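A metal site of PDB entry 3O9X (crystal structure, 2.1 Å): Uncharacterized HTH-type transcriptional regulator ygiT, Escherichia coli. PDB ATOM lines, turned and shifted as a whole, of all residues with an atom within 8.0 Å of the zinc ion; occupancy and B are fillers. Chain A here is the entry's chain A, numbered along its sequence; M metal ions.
The side-chain sulfur (SG) of Cys 8 sits close to a ring nitrogen (ND1) of His 41, at 3.6 Å.
The backbone NH (N) of Gly 11 sits close to the side-chain sulfur (SG) of Cys 8, 3.7 Å away.
The side-chain sulfur (SG) of Cys 8 lies close to the backbone NH (N) of Gln 10, 3.4 Å away.
The side-chain sulfur (SG) of Cys 42 sits close to the backbone NH (N) of Glu 44 (3.4 Å).
The backbone carbonyl oxygen (O) of Glu 44 sits at hydrogen-bond distance from the backbone NH (N) of Cys 39, at 3.0 Å.
The backbone NH of His 41 lies close to the side-chain sulfur of Cys 39 (3.1 Å).
N of Cys 5 is in hydrogen-bond range of O of Gly 11, 2.8 Å away.
The backbone carbonyl oxygen of Cys 5 sits close to a ring nitrogen (ND1) of His 9 (3.2 Å).
Of the 18 residues printed, 4 come within 4 Å of the zinc ion.
The nearest printed residue that does not touch the zinc ion is Glu 44 (4.2 Å).
The zinc ion is bound by the side-chain sulfur of Cys 8 (2.2 Å), the side-chain sulfur of Cys 42 (2.3 Å), the side-chain sulfur of Cys 39 (2.3 Å) and the side-chain sulfur of Cys 5 (2.3 Å).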
ATOM      1  N   LYS A   4     -11.134 -12.270   3.419  1.00  0.00           N
ATOM      2  CA  LYS A   4      -9.694 -12.223   3.534  1.00  0.00           C
ATOM      3  C   LYS A   4      -9.039 -12.428   2.165  1.00  0.00           C
ATOM      4  O   LYS A   4      -9.592 -13.133   1.297  1.00  0.00           O
ATOM      5  CB  LYS A   4      -9.212 -13.286   4.543  1.00  0.00           C
ATOM      6  CG  LYS A   4      -7.699 -13.393   4.668  1.00  0.00           C
ATOM      7  N   CYS A   5      -7.883 -11.807   1.963  1.00  0.00           N
ATOM      8  CA  CYS A   5      -7.127 -11.958   0.729  1.00  0.00           C
ATOM      9  C   CYS A   5      -6.741 -13.416   0.514  1.00  0.00           C
ATOM     10  O   CYS A   5      -6.002 -13.981   1.332  1.00  0.00           O
ATOM     11  CB  CYS A   5      -5.862 -11.105   0.788  1.00  0.00           C
ATOM     12  SG  CYS A   5      -4.814 -11.235  -0.663  1.00  0.00           S
ATOM     13  N   PRO A   6      -7.250 -14.039  -0.564  1.00  0.00           N
ATOM     14  CA  PRO A   6      -6.946 -15.432  -0.899  1.00  0.00           C
ATOM     15  C   PRO A   6      -5.494 -15.639  -1.315  1.00  0.00           C
ATOM     16  O   PRO A   6      -5.114 -16.783  -1.575  1.00  0.00           O
ATOM     17  CB  PRO A   6      -7.863 -15.724  -2.086  1.00  0.00           C
ATOM     18  CG  PRO A   6      -8.153 -14.395  -2.678  1.00  0.00           C
ATOM     19  CD  PRO A   6      -8.187 -13.441  -1.526  1.00  0.00           C
ATOM     20  N   VAL A   7      -4.704 -14.568  -1.378  1.00  0.00           N
ATOM     21  CA  VAL A   7      -3.305 -14.661  -1.806  1.00  0.00           C
ATOM     22  C   VAL A   7      -2.330 -14.575  -0.632  1.00  0.00           C
ATOM     23  O   VAL A   7      -1.612 -15.536  -0.347  1.00  0.00           O
ATOM     24  CB  VAL A   7      -2.946 -13.578  -2.849  1.00  0.00           C
ATOM     25  CG1 VAL A   7      -1.463 -13.585  -3.137  1.00  0.00           C
ATOM     26  CG2 VAL A   7      -3.720 -13.813  -4.132  1.00  0.00           C
ATOM     27  N   CYS A   8      -2.293 -13.448   0.056  1.00  0.00           N
ATOM     28  CA  CYS A   8      -1.389 -13.291   1.191  1.00  0.00           C
ATOM     29  C   CYS A   8      -2.020 -13.718   2.513  1.00  0.00           C
ATOM     30  O   CYS A   8      -1.314 -13.942   3.489  1.00  0.00           O
ATOM     31  CB  CYS A   8      -0.832 -11.863   1.282  1.00  0.00           C
ATOM     32  SG  CYS A   8      -2.010 -10.586   1.847  1.00  0.00           S
ATOM     33  N   HIS A   9      -3.351 -13.847   2.534  1.00  0.00           N
ATOM     34  CA  HIS A   9      -4.062 -14.263   3.742  1.00  0.00           C
ATOM     35  C   HIS A   9      -3.826 -13.314   4.913  1.00  0.00           C
ATOM     36  O   HIS A   9      -4.194 -13.626   6.043  1.00  0.00           O
ATOM     37  CB  HIS A   9      -3.621 -15.664   4.181  1.00  0.00           C
ATOM     38  CG  HIS A   9      -3.677 -16.707   3.112  1.00  0.00           C
ATOM     39  ND1 HIS A   9      -4.730 -16.795   2.221  1.00  0.00           N
ATOM     40  CD2 HIS A   9      -2.811 -17.690   2.779  1.00  0.00           C
ATOM     41  CE1 HIS A   9      -4.503 -17.808   1.388  1.00  0.00           C
ATOM     42  NE2 HIS A   9      -3.354 -18.360   1.702  1.00  0.00           N
ATOM     43  N   GLN A  10      -3.218 -12.164   4.641  1.00  0.00           N
ATOM     44  CA  GLN A  10      -2.812 -11.221   5.689  1.00  0.00           C
ATOM     45  C   GLN A  10      -3.562  -9.881   5.618  1.00  0.00           C
ATOM     46  O   GLN A  10      -3.433  -9.049   6.526  1.00  0.00           O
ATOM     47  CB  GLN A  10      -1.308 -10.963   5.628  1.00  0.00           C
ATOM     48  CG  GLN A  10      -0.455 -12.165   5.986  1.00  0.00           C
ATOM     49  CD  GLN A  10       1.035 -11.832   5.974  1.00  0.00           C
ATOM     50  OE1 GLN A  10       1.416 -10.669   5.912  1.00  0.00           O
ATOM     51  NE2 GLN A  10       1.866 -12.866   6.035  1.00  0.00           N
ATOM     52  N   GLY A  11      -4.315  -9.681   4.553  1.00  0.00           N
ATOM     53  CA  GLY A  11      -5.114  -8.468   4.425  1.00  0.00           C
ATOM     54  C   GLY A  11      -6.546  -8.817   4.129  1.00  0.00           C
ATOM     55  O   GLY A  11      -6.861  -9.913   3.681  1.00  0.00           O
ATOM     56  N   GLU A  12      -7.435  -7.872   4.398  1.00  0.00           N
ATOM     57  CA  GLU A  12      -8.841  -7.992   4.051  1.00  0.00           C
ATOM     58  C   GLU A  12      -9.030  -7.391   2.665  1.00  0.00           C
ATOM     59  O   GLU A  12      -8.264  -6.505   2.271  1.00  0.00           O
ATOM     60  CB  GLU A  12      -9.648  -7.212   5.077  1.00  0.00           C
ATOM     61  CG  GLU A  12     -10.999  -7.806   5.417  1.00  0.00           C
ATOM     62  CD  GLU A  12     -11.636  -7.135   6.623  1.00  0.00           C
ATOM     63  OE1 GLU A  12     -12.558  -6.315   6.426  1.00  0.00           O
ATOM     64  OE2 GLU A  12     -11.209  -7.431   7.770  1.00  0.00           O
ATOM     65  N   MET A  13     -10.029  -7.869   1.919  1.00  0.00           N
ATOM     66  CA  MET A  13     -10.426  -7.277   0.657  1.00  0.00           C
ATOM     67  C   MET A  13     -11.395  -6.142   0.923  1.00  0.00           C
ATOM     68  O   MET A  13     -12.483  -6.370   1.464  1.00  0.00           O
ATOM     69  CB  MET A  13     -11.092  -8.300  -0.278  1.00  0.00           C
ATOM     70  CG  MET A  13     -10.264  -9.544  -0.589  1.00  0.00           C
ATOM     71  SD  MET A  13      -8.600  -9.226  -1.200  1.00  0.00           S
ATOM     72  CE  MET A  13      -8.920  -8.339  -2.717  1.00  0.00           C
ATOM     73  N   TYR A  38      -9.793  -4.618  -3.031  1.00  0.00           N
ATOM     74  CA  TYR A  38      -8.337  -4.601  -2.968  1.00  0.00           C
ATOM     75  C   TYR A  38      -7.872  -5.078  -1.614  1.00  0.00           C
ATOM     76  O   TYR A  38      -8.463  -4.735  -0.599  1.00  0.00           O
ATOM     77  CB  TYR A  38      -7.788  -3.203  -3.262  1.00  0.00           C
ATOM     78  CG  TYR A  38      -8.110  -2.724  -4.651  1.00  0.00           C
ATOM     79  CD1 TYR A  38      -7.361  -3.139  -5.748  1.00  0.00           C
ATOM     80  CD2 TYR A  38      -9.175  -1.853  -4.875  1.00  0.00           C
ATOM     81  CE1 TYR A  38      -7.662  -2.709  -7.034  1.00  0.00           C
ATOM     82  CE2 TYR A  38      -9.482  -1.411  -6.156  1.00  0.00           C
ATOM     83  CZ  TYR A  38      -8.727  -1.850  -7.233  1.00  0.00           C
ATOM     84  OH  TYR A  38      -9.016  -1.424  -8.513  1.00  0.00           O
ATOM     85  N   CYS A  39      -6.810  -5.879  -1.614  1.00  0.00           N
ATOM     86  CA  CYS A  39      -6.243  -6.345  -0.369  1.00  0.00           C
ATOM     87  C   CYS A  39      -5.512  -5.192   0.315  1.00  0.00           C
ATOM     88  O   CYS A  39      -4.750  -4.458  -0.324  1.00  0.00           O
ATOM     89  CB  CYS A  39      -5.289  -7.514  -0.597  1.00  0.00           C
ATOM     90  SG  CYS A  39      -4.480  -8.058   0.936  1.00  0.00           S
ATOM     91  N   VAL A  40      -5.749  -5.062   1.615  1.00  0.00           N
ATOM     92  CA  VAL A  40      -5.086  -4.064   2.422  1.00  0.00           C
ATOM     93  C   VAL A  40      -3.593  -4.305   2.425  1.00  0.00           C
ATOM     94  O   VAL A  40      -2.806  -3.361   2.491  1.00  0.00           O
ATOM     95  CB  VAL A  40      -5.579  -4.118   3.881  1.00  0.00           C
ATOM     96  CG1 VAL A  40      -4.578  -3.421   4.794  1.00  0.00           C
ATOM     97  CG2 VAL A  40      -6.964  -3.508   4.005  1.00  0.00           C
ATOM     98  N   HIS A  41      -3.205  -5.573   2.341  1.00  0.00           N
ATOM     99  CA  HIS A  41      -1.819  -5.972   2.543  1.00  0.00           C
ATOM    100  C   HIS A  41      -0.989  -6.068   1.264  1.00  0.00           C
ATOM    101  O   HIS A  41       0.106  -5.514   1.171  1.00  0.00           O
ATOM    102  CB  HIS A  41      -1.756  -7.311   3.295  1.00  0.00           C
ATOM    103  CG  HIS A  41      -0.382  -7.702   3.724  1.00  0.00           C
ATOM    104  ND1 HIS A  41       0.544  -8.245   2.861  1.00  0.00           N
ATOM    105  CD2 HIS A  41       0.220  -7.644   4.940  1.00  0.00           C
ATOM    106  CE1 HIS A  41       1.660  -8.500   3.515  1.00  0.00           C
ATOM    107  NE2 HIS A  41       1.493  -8.147   4.783  1.00  0.00           N
ATOM    108  N   CYS A  42      -1.505  -6.784   0.268  1.00  0.00           N
ATOM    109  CA  CYS A  42      -0.765  -6.992  -0.977  1.00  0.00           C
ATOM    110  C   CYS A  42      -1.509  -6.402  -2.163  1.00  0.00           C
ATOM    111  O   CYS A  42      -2.406  -5.571  -2.006  1.00  0.00           O
ATOM    112  CB  CYS A  42      -0.462  -8.480  -1.214  1.00  0.00           C
ATOM    113  SG  CYS A  42      -1.889  -9.491  -1.657  1.00  0.00           S
ATOM    114  N   GLU A  43      -1.129  -6.857  -3.348  1.00  0.00           N
ATOM    115  CA  GLU A  43      -1.632  -6.304  -4.607  1.00  0.00           C
ATOM    116  C   GLU A  43      -2.860  -7.037  -5.115  1.00  0.00           C
ATOM    117  O   GLU A  43      -3.461  -6.645  -6.115  1.00  0.00           O
ATOM    118  CB  GLU A  43      -0.544  -6.357  -5.675  1.00  0.00           C
ATOM    119  CG  GLU A  43       0.715  -5.607  -5.282  1.00  0.00           C
ATOM    120  CD  GLU A  43       0.459  -4.118  -5.105  1.00  0.00           C
ATOM    121  OE1 GLU A  43      -0.548  -3.624  -5.658  1.00  0.00           O
ATOM    122  OE2 GLU A  43       1.241  -3.445  -4.417  1.00  0.00           O
ATOM    123  N   GLU A  44      -3.226  -8.116  -4.435  1.00  0.00           N
ATOM    124  CA  GLU A  44      -4.393  -8.895  -4.815  1.00  0.00           C
ATOM    125  C   GLU A  44      -5.600  -7.988  -4.995  1.00  0.00           C
ATOM    126  O   GLU A  44      -5.925  -7.196  -4.108  1.00  0.00           O
ATOM    127  CB  GLU A  44      -4.691  -9.954  -3.744  1.00  0.00           C
ATOM    128  CG  GLU A  44      -5.986 -10.705  -3.937  1.00  0.00           C
ATOM    129  CD  GLU A  44      -5.985 -11.578  -5.161  1.00  0.00           C
ATOM    130  OE1 GLU A  44      -4.967 -11.581  -5.891  1.00  0.00           O
ATOM    131  OE2 GLU A  44      -6.993 -12.264  -5.397  1.00  0.00           O
ATOM    132  N   SER A  45      -6.252  -8.094  -6.148  1.00  0.00           N
ATOM    133  CA  SER A  45      -7.495  -7.376  -6.406  1.00  0.00           C
ATOM    134  C   SER A  45      -8.553  -8.339  -6.920  1.00  0.00           C
ATOM    135  O   SER A  45      -8.250  -9.337  -7.582  1.00  0.00           O
ATOM    136  CB  SER A  45      -7.291  -6.252  -7.411  1.00  0.00           C
ATOM    137  OG  SER A  45      -7.342  -6.730  -8.747  1.00  0.00           O
HETATM  138 ZN    ZN M   1      -3.180  -9.820   0.181  1.00  0.00          ZN
